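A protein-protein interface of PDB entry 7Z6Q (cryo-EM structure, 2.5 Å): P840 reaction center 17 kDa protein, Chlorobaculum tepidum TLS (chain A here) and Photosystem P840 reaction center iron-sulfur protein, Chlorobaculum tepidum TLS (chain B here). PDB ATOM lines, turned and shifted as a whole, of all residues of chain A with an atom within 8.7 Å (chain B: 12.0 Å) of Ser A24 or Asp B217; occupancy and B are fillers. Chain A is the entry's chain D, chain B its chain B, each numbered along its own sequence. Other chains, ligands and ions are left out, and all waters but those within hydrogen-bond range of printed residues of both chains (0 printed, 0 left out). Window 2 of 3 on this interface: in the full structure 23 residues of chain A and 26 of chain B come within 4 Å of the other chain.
The side-chain carboxylate (OD2) of Asp B207 lies within hydrogen-bond range of the side-chain amide nitrogen (ND2) of Asn A26. OG of Ser A24 lies within hydrogen-bond range of OD2 of Asp B217, at 3.4 Å. The side-chain carboxylate (OD2) of Asp B207 is in hydrogen-bond range of a ring nitrogen (NE2) of His A29.
ND2 of Asn A26 sits at hydrogen-bond distance from NE2 of His A29, at 3.2 Å.
Among the printed residues, merely in contact across the chains: Ser A24 with Arg B215, Gly A25 with Pro B212, Gly A25 with Pro B213, Asn A26 with Thr B211 and Glu A32 with Glu B214.
No residue of chain B comes within 4 Å of Ser A20. Gly A21 touches none of the printed residues of chain B. No residue of chain B comes within 4 Å of Pro A22. No residue of chain B comes within 4 Å of Trp A23. Ser A24 touches just these residues of chain B: Arg B215 and Asp B217. Ala A27 touches none of the printed residues of chain B. Of the printed residues of chain B, Glu A32 touches Glu B214 (3.9 Å). Printed residues of chain A within 4 Å of Thr B211: Asn A26. Printed residues of chain A within 4 Å of Pro B212: Gly A25. Asp B217 touches one residue of chain A. Asp B219 touches none of the printed residues of chain A.
Of the 14 printed residues of chain A, 5 touch a printed residue of chain B. Of the 14 printed residues of chain B, 7 touch a printed residue of chain A.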
ATOM      1  N   VAL A  19      -5.731  -7.190 -15.117  1.00  0.00           N
ATOM      2  CA  VAL A  19      -4.343  -6.803 -15.294  1.00  0.00           C
ATOM      3  C   VAL A  19      -3.957  -5.841 -14.188  1.00  0.00           C
ATOM      4  O   VAL A  19      -4.783  -5.076 -13.706  1.00  0.00           O
ATOM      5  CB  VAL A  19      -4.092  -6.098 -16.640  1.00  0.00           C
ATOM      6  CG1 VAL A  19      -4.364  -7.050 -17.795  1.00  0.00           C
ATOM      7  CG2 VAL A  19      -4.924  -4.833 -16.764  1.00  0.00           C
ATOM      8  N   SER A  20      -2.701  -5.904 -13.765  1.00  0.00           N
ATOM      9  CA  SER A  20      -2.196  -4.997 -12.747  1.00  0.00           C
ATOM     10  C   SER A  20      -1.947  -3.626 -13.370  1.00  0.00           C
ATOM     11  O   SER A  20      -1.795  -3.496 -14.588  1.00  0.00           O
ATOM     12  CB  SER A  20      -0.919  -5.538 -12.109  1.00  0.00           C
ATOM     13  OG  SER A  20       0.150  -5.558 -13.037  1.00  0.00           O
ATOM     14  N   GLY A  21      -1.899  -2.602 -12.514  1.00  0.00           N
ATOM     15  CA  GLY A  21      -1.699  -1.211 -12.962  1.00  0.00           C
ATOM     16  C   GLY A  21      -0.273  -0.918 -13.396  1.00  0.00           C
ATOM     17  O   GLY A  21       0.628  -1.737 -13.131  1.00  0.00           O
ATOM     18  N   PRO A  22       0.004   0.259 -13.994  1.00  0.00           N
ATOM     19  CA  PRO A  22       1.354   0.600 -14.439  1.00  0.00           C
ATOM     20  C   PRO A  22       2.314   0.649 -13.242  1.00  0.00           C
ATOM     21  O   PRO A  22       3.439   0.224 -13.375  1.00  0.00           O
ATOM     22  CB  PRO A  22       1.202   2.008 -15.029  1.00  0.00           C
ATOM     23  CG  PRO A  22      -0.269   2.121 -15.352  1.00  0.00           C
ATOM     24  CD  PRO A  22      -0.962   1.320 -14.273  1.00  0.00           C
ATOM     25  N   TRP A  23       1.836   1.171 -12.111  1.00  0.00           N
ATOM     26  CA  TRP A  23       2.652   1.312 -10.878  1.00  0.00           C
ATOM     27  C   TRP A  23       3.107  -0.054 -10.353  1.00  0.00           C
ATOM     28  O   TRP A  23       4.263  -0.136  -9.905  1.00  0.00           O
ATOM     29  CB  TRP A  23       1.881   2.144  -9.851  1.00  0.00           C
ATOM     30  CG  TRP A  23       1.299   3.361 -10.499  1.00  0.00           C
ATOM     31  CD1 TRP A  23       1.978   4.311 -11.203  1.00  0.00           C
ATOM     32  CD2 TRP A  23      -0.089   3.734 -10.561  1.00  0.00           C
ATOM     33  NE1 TRP A  23       1.116   5.260 -11.678  1.00  0.00           N
ATOM     34  CE2 TRP A  23      -0.160   4.932 -11.299  1.00  0.00           C
ATOM     35  CE3 TRP A  23      -1.271   3.182 -10.058  1.00  0.00           C
ATOM     36  CZ2 TRP A  23      -1.364   5.587 -11.541  1.00  0.00           C
ATOM     37  CZ3 TRP A  23      -2.462   3.830 -10.299  1.00  0.00           C
ATOM     38  CH2 TRP A  23      -2.505   5.016 -11.031  1.00  0.00           C
ATOM     39  N   SER A  24       2.252  -1.081 -10.396  1.00  0.00           N
ATOM     40  CA  SER A  24       2.693  -2.417  -9.914  1.00  0.00           C
ATOM     41  C   SER A  24       3.642  -3.030 -10.950  1.00  0.00           C
ATOM     42  O   SER A  24       3.247  -3.131 -12.124  1.00  0.00           O
ATOM     43  CB  SER A  24       1.519  -3.319  -9.654  1.00  0.00           C
ATOM     44  OG  SER A  24       0.606  -2.711  -8.755  1.00  0.00           O
ATOM     45  N   GLY A  25       4.834  -3.452 -10.517  1.00  0.00           N
ATOM     46  CA  GLY A  25       5.843  -4.028 -11.429  1.00  0.00           C
ATOM     47  C   GLY A  25       6.336  -3.006 -12.440  1.00  0.00           C
ATOM     48  O   GLY A  25       6.382  -1.811 -12.103  1.00  0.00           O
ATOM     49  N   ASN A  26       6.741  -3.463 -13.626  1.00  0.00           N
ATOM     50  CA  ASN A  26       7.201  -2.530 -14.690  1.00  0.00           C
ATOM     51  C   ASN A  26       5.983  -1.781 -15.241  1.00  0.00           C
ATOM     52  O   ASN A  26       4.901  -2.392 -15.301  1.00  0.00           O
ATOM     53  CB  ASN A  26       7.983  -3.250 -15.791  1.00  0.00           C
ATOM     54  CG  ASN A  26       9.033  -2.370 -16.432  1.00  0.00           C
ATOM     55  OD1 ASN A  26       9.168  -1.203 -16.079  1.00  0.00           O
ATOM     56  ND2 ASN A  26       9.783  -2.919 -17.371  1.00  0.00           N
ATOM     57  N   ALA A  27       6.158  -0.514 -15.629  1.00  0.00           N
ATOM     58  CA  ALA A  27       5.038   0.295 -16.164  1.00  0.00           C
ATOM     59  C   ALA A  27       4.836  -0.008 -17.651  1.00  0.00           C
ATOM     60  O   ALA A  27       3.676  -0.121 -18.085  1.00  0.00           O
ATOM     61  CB  ALA A  27       5.307   1.759 -15.930  1.00  0.00           C
ATOM     62  N   VAL A  28       5.934  -0.137 -18.398  1.00  0.00           N
ATOM     63  CA  VAL A  28       5.845  -0.421 -19.863  1.00  0.00           C
ATOM     64  C   VAL A  28       5.054  -1.711 -20.131  1.00  0.00           C
ATOM     65  O   VAL A  28       4.254  -1.714 -21.085  1.00  0.00           O
ATOM     66  CB  VAL A  28       7.237  -0.451 -20.527  1.00  0.00           C
ATOM     67  CG1 VAL A  28       7.863   0.932 -20.577  1.00  0.00           C
ATOM     68  CG2 VAL A  28       8.181  -1.433 -19.855  1.00  0.00           C
ATOM     69  N   HIS A  29       5.267  -2.752 -19.318  1.00  0.00           N
ATOM     70  CA  HIS A  29       4.603  -4.071 -19.498  1.00  0.00           C
ATOM     71  C   HIS A  29       3.099  -3.993 -19.203  1.00  0.00           C
ATOM     72  O   HIS A  29       2.716  -3.256 -18.281  1.00  0.00           O
ATOM     73  CB  HIS A  29       5.285  -5.128 -18.617  1.00  0.00           C
ATOM     74  CG  HIS A  29       6.758  -5.245 -18.824  1.00  0.00           C
ATOM     75  ND1 HIS A  29       7.406  -4.664 -19.892  1.00  0.00           N
ATOM     76  CD2 HIS A  29       7.711  -5.876 -18.105  1.00  0.00           C
ATOM     77  CE1 HIS A  29       8.694  -4.931 -19.825  1.00  0.00           C
ATOM     78  NE2 HIS A  29       8.907  -5.674 -18.738  1.00  0.00           N
ATOM     79  N   LYS A  30       2.273  -4.762 -19.914  1.00  0.00           N
ATOM     80  CA  LYS A  30       0.809  -4.831 -19.653  1.00  0.00           C
ATOM     81  C   LYS A  30       0.497  -6.131 -18.903  1.00  0.00           C
ATOM     82  O   LYS A  30      -0.565  -6.241 -18.236  1.00  0.00           O
ATOM     83  CB  LYS A  30       0.036  -4.930 -20.961  1.00  0.00           C
ATOM     84  CG  LYS A  30      -1.433  -4.576 -20.860  1.00  0.00           C
ATOM     85  CD  LYS A  30      -1.623  -3.113 -21.097  1.00  0.00           C
ATOM     86  CE  LYS A  30      -1.347  -2.717 -22.523  1.00  0.00           C
ATOM     87  NZ  LYS A  30      -1.422  -1.252 -22.694  1.00  0.00           N
ATOM     88  N   ALA A  31       1.381  -7.100 -19.115  1.00  0.00           N
ATOM     89  CA  ALA A  31       1.419  -8.434 -18.481  1.00  0.00           C
ATOM     90  C   ALA A  31       2.889  -8.687 -18.184  1.00  0.00           C
ATOM     91  O   ALA A  31       3.736  -8.231 -18.966  1.00  0.00           O
ATOM     92  CB  ALA A  31       0.907  -9.469 -19.439  1.00  0.00           C
ATOM     93  N   GLU A  32       3.177  -9.520 -17.197  1.00  0.00           N
ATOM     94  CA  GLU A  32       4.550  -9.819 -16.814  1.00  0.00           C
ATOM     95  C   GLU A  32       5.287 -10.505 -17.958  1.00  0.00           C
ATOM     96  O   GLU A  32       4.700 -11.227 -18.767  1.00  0.00           O
ATOM     97  CB  GLU A  32       4.592 -10.684 -15.557  1.00  0.00           C
ATOM     98  CG  GLU A  32       5.739 -10.321 -14.625  1.00  0.00           C
ATOM     99  CD  GLU A  32       5.717 -11.100 -13.328  1.00  0.00           C
ATOM    100  OE1 GLU A  32       4.623 -11.259 -12.749  1.00  0.00           O
ATOM    101  OE2 GLU A  32       6.794 -11.550 -12.882  1.00  0.00           O
ATOM    102  N   ASP B 207      15.646  -5.860 -18.242  1.00  0.00           N
ATOM    103  CA  ASP B 207      15.110  -4.783 -19.112  1.00  0.00           C
ATOM    104  C   ASP B 207      15.279  -3.419 -18.435  1.00  0.00           C
ATOM    105  O   ASP B 207      15.340  -2.421 -19.162  1.00  0.00           O
ATOM    106  CB  ASP B 207      13.653  -5.045 -19.490  1.00  0.00           C
ATOM    107  CG  ASP B 207      12.674  -4.689 -18.391  1.00  0.00           C
ATOM    108  OD1 ASP B 207      13.050  -4.808 -17.210  1.00  0.00           O
ATOM    109  OD2 ASP B 207      11.546  -4.308 -18.727  1.00  0.00           O
ATOM    110  N   PHE B 208      15.355  -3.385 -17.102  1.00  0.00           N
ATOM    111  CA  PHE B 208      15.499  -2.148 -16.355  1.00  0.00           C
ATOM    112  C   PHE B 208      16.353  -2.417 -15.125  1.00  0.00           C
ATOM    113  O   PHE B 208      16.390  -3.539 -14.613  1.00  0.00           O
ATOM    114  CB  PHE B 208      14.123  -1.595 -15.957  1.00  0.00           C
ATOM    115  CG  PHE B 208      14.127  -0.141 -15.589  1.00  0.00           C
ATOM    116  CD1 PHE B 208      14.246   0.835 -16.564  1.00  0.00           C
ATOM    117  CD2 PHE B 208      13.986   0.254 -14.275  1.00  0.00           C
ATOM    118  CE1 PHE B 208      14.237   2.175 -16.228  1.00  0.00           C
ATOM    119  CE2 PHE B 208      13.977   1.588 -13.932  1.00  0.00           C
ATOM    120  CZ  PHE B 208      14.101   2.550 -14.909  1.00  0.00           C
ATOM    121  N   TYR B 210      16.185  -1.459 -11.965  1.00  0.00           N
ATOM    122  CA  TYR B 210      15.457  -1.899 -10.781  1.00  0.00           C
ATOM    123  C   TYR B 210      13.972  -1.918 -11.107  1.00  0.00           C
ATOM    124  O   TYR B 210      13.456  -0.961 -11.686  1.00  0.00           O
ATOM    125  CB  TYR B 210      15.713  -0.986  -9.573  1.00  0.00           C
ATOM    126  CG  TYR B 210      14.597  -1.063  -8.552  1.00  0.00           C
ATOM    127  CD1 TYR B 210      14.514  -2.131  -7.670  1.00  0.00           C
ATOM    128  CD2 TYR B 210      13.610  -0.087  -8.494  1.00  0.00           C
ATOM    129  CE1 TYR B 210      13.490  -2.220  -6.753  1.00  0.00           C
ATOM    130  CE2 TYR B 210      12.582  -0.170  -7.581  1.00  0.00           C
ATOM    131  CZ  TYR B 210      12.527  -1.237  -6.712  1.00  0.00           C
ATOM    132  OH  TYR B 210      11.505  -1.322  -5.797  1.00  0.00           O
ATOM    133  N   THR B 211      13.283  -2.982 -10.707  1.00  0.00           N
ATOM    134  CA  THR B 211      11.869  -3.101 -11.017  1.00  0.00           C
ATOM    135  C   THR B 211      11.032  -3.024  -9.750  1.00  0.00           C
ATOM    136  O   THR B 211      11.315  -3.741  -8.781  1.00  0.00           O
ATOM    137  CB  THR B 211      11.585  -4.417 -11.752  1.00  0.00           C
ATOM    138  OG1 THR B 211      12.496  -4.557 -12.849  1.00  0.00           O
ATOM    139  CG2 THR B 211      10.159  -4.433 -12.283  1.00  0.00           C
ATOM    140  N   PRO B 212      10.010  -2.170  -9.719  1.00  0.00           N
ATOM    141  CA  PRO B 212       9.171  -2.076  -8.527  1.00  0.00           C
ATOM    142  C   PRO B 212       8.468  -3.388  -8.253  1.00  0.00           C
ATOM    143  O   PRO B 212       8.165  -4.160  -9.182  1.00  0.00           O
ATOM    144  CB  PRO B 212       8.171  -0.967  -8.887  1.00  0.00           C
ATOM    145  CG  PRO B 212       8.840  -0.160  -9.932  1.00  0.00           C
ATOM    146  CD  PRO B 212       9.785  -1.061 -10.662  1.00  0.00           C
ATOM    147  N   PRO B 213       8.184  -3.685  -6.985  1.00  0.00           N
ATOM    148  CA  PRO B 213       7.543  -4.962  -6.647  1.00  0.00           C
ATOM    149  C   PRO B 213       6.079  -5.005  -7.058  1.00  0.00           C
ATOM    150  O   PRO B 213       5.355  -4.012  -6.979  1.00  0.00           O
ATOM    151  CB  PRO B 213       7.682  -5.038  -5.120  1.00  0.00           C
ATOM    152  CG  PRO B 213       8.655  -3.950  -4.744  1.00  0.00           C
ATOM    153  CD  PRO B 213       8.513  -2.901  -5.786  1.00  0.00           C
ATOM    154  N   GLU B 214       5.642  -6.194  -7.471  1.00  0.00           N
ATOM    155  CA  GLU B 214       4.253  -6.403  -7.860  1.00  0.00           C
ATOM    156  C   GLU B 214       3.325  -6.352  -6.649  1.00  0.00           C
ATOM    157  O   GLU B 214       3.711  -6.682  -5.526  1.00  0.00           O
ATOM    158  CB  GLU B 214       4.094  -7.740  -8.586  1.00  0.00           C
ATOM    159  CG  GLU B 214       4.632  -7.761 -10.014  1.00  0.00           C
ATOM    160  CD  GLU B 214       6.146  -7.865 -10.088  1.00  0.00           C
ATOM    161  OE1 GLU B 214       6.809  -7.806  -9.032  1.00  0.00           O
ATOM    162  OE2 GLU B 214       6.674  -8.007 -11.212  1.00  0.00           O
ATOM    163  N   ARG B 215       2.082  -5.928  -6.893  1.00  0.00           N
ATOM    164  CA  ARG B 215       1.079  -5.745  -5.851  1.00  0.00           C
ATOM    165  C   ARG B 215      -0.287  -6.172  -6.379  1.00  0.00           C
ATOM    166  O   ARG B 215      -0.533  -6.133  -7.586  1.00  0.00           O
ATOM    167  CB  ARG B 215       0.985  -4.272  -5.406  1.00  0.00           C
ATOM    168  CG  ARG B 215       2.309  -3.537  -5.239  1.00  0.00           C
ATOM    169  CD  ARG B 215       2.998  -3.910  -3.953  1.00  0.00           C
ATOM    170  NE  ARG B 215       2.096  -3.799  -2.812  1.00  0.00           N
ATOM    171  CZ  ARG B 215       2.085  -2.776  -1.965  1.00  0.00           C
ATOM    172  NH1 ARG B 215       2.935  -1.776  -2.123  1.00  0.00           N
ATOM    173  NH2 ARG B 215       1.229  -2.759  -0.954  1.00  0.00           N
ATOM    174  N   LEU B 216      -1.178  -6.572  -5.469  1.00  0.00           N
ATOM    175  CA  LEU B 216      -2.604  -6.539  -5.775  1.00  0.00           C
ATOM    176  C   LEU B 216      -3.070  -5.088  -5.885  1.00  0.00           C
ATOM    177  O   LEU B 216      -2.321  -4.156  -5.580  1.00  0.00           O
ATOM    178  CB  LEU B 216      -3.429  -7.280  -4.707  1.00  0.00           C
ATOM    179  CG  LEU B 216      -3.379  -8.787  -4.392  1.00  0.00           C
ATOM    180  CD1 LEU B 216      -4.178  -9.238  -3.214  1.00  0.00           C
ATOM    181  CD2 LEU B 216      -3.866  -9.548  -5.620  1.00  0.00           C
ATOM    182  N   ASP B 217      -4.334  -4.889  -6.286  1.00  0.00           N
ATOM    183  CA  ASP B 217      -4.917  -3.547  -6.211  1.00  0.00           C
ATOM    184  C   ASP B 217      -6.377  -3.558  -5.765  1.00  0.00           C
ATOM    185  O   ASP B 217      -7.200  -4.296  -6.314  1.00  0.00           O
ATOM    186  CB  ASP B 217      -4.696  -2.762  -7.499  1.00  0.00           C
ATOM    187  CG  ASP B 217      -3.359  -2.040  -7.474  1.00  0.00           C
ATOM    188  OD1 ASP B 217      -2.999  -1.547  -6.376  1.00  0.00           O
ATOM    189  OD2 ASP B 217      -2.668  -1.969  -8.510  1.00  0.00           O
ATOM    190  N   PHE B 218      -6.662  -2.773  -4.712  1.00  0.00           N
ATOM    191  CA  PHE B 218      -8.014  -2.417  -4.289  1.00  0.00           C
ATOM    192  C   PHE B 218      -8.025  -1.027  -3.660  1.00  0.00           C
ATOM    193  O   PHE B 218      -7.040  -0.566  -3.078  1.00  0.00           O
ATOM    194  CB  PHE B 218      -8.647  -3.413  -3.296  1.00  0.00           C
ATOM    195  CG  PHE B 218      -8.206  -3.245  -1.850  1.00  0.00           C
ATOM    196  CD1 PHE B 218      -8.963  -2.487  -0.963  1.00  0.00           C
ATOM    197  CD2 PHE B 218      -7.158  -3.989  -1.335  1.00  0.00           C
ATOM    198  CE1 PHE B 218      -8.608  -2.370   0.370  1.00  0.00           C
ATOM    199  CE2 PHE B 218      -6.805  -3.887   0.004  1.00  0.00           C
ATOM    200  CZ  PHE B 218      -7.531  -3.075   0.855  1.00  0.00           C
ATOM    201  N   ASP B 219      -9.160  -0.340  -3.823  1.00  0.00           N
ATOM    202  CA  ASP B 219      -9.354   1.019  -3.251  1.00  0.00           C
ATOM    203  C   ASP B 219     -10.038   0.858  -1.890  1.00  0.00           C
ATOM    204  O   ASP B 219     -11.040   0.124  -1.823  1.00  0.00           O
ATOM    205  CB  ASP B 219     -10.152   1.917  -4.198  1.00  0.00           C
ATOM    206  CG  ASP B 219     -10.296   3.347  -3.701  1.00  0.00           C
ATOM    207  OD1 ASP B 219      -9.754   3.650  -2.618  1.00  0.00           O
ATOM    208  OD2 ASP B 219     -10.947   4.147  -4.404  1.00  0.00           O
ATOM    209  N   LEU B 220      -9.529   1.531  -0.856  1.00  0.00           N
ATOM    210  CA  LEU B 220     -10.128   1.375   0.493  1.00  0.00           C
ATOM    211  C   LEU B 220     -11.210   2.437   0.719  1.00  0.00           C
ATOM    212  O   LEU B 220     -10.877   3.634   0.770  1.00  0.00           O
ATOM    213  CB  LEU B 220      -9.021   1.484   1.546  1.00  0.00           C
ATOM    214  CG  LEU B 220      -9.490   1.452   2.999  1.00  0.00           C
ATOM    215  CD1 LEU B 220      -9.963   0.062   3.386  1.00  0.00           C
ATOM    216  CD2 LEU B 220      -8.387   1.917   3.933  1.00  0.00           C
ATOM    217  N   ARG B 221     -12.453   2.002   0.935  1.00  0.00           N
ATOM    218  CA  ARG B 221     -13.564   2.927   1.294  1.00  0.00           C
ATOM    219  C   ARG B 221     -13.921   2.704   2.774  1.00  0.00           C
ATOM    220  O   ARG B 221     -13.342   1.792   3.391  1.00  0.00           O
ATOM    221  CB  ARG B 221     -14.759   2.761   0.352  1.00  0.00           C
ATOM    222  CG  ARG B 221     -14.500   3.243  -1.068  1.00  0.00           C
ATOM    223  CD  ARG B 221     -15.659   3.011  -2.014  1.00  0.00           C
ATOM    224  NE  ARG B 221     -16.693   4.027  -1.886  1.00  0.00           N
ATOM    225  CZ  ARG B 221     -16.922   4.982  -2.780  1.00  0.00           C
ATOM    226  NH1 ARG B 221     -17.883   5.863  -2.575  1.00  0.00           N
ATOM    227  NH2 ARG B 221     -16.188   5.049  -3.873  1.00  0.00           N
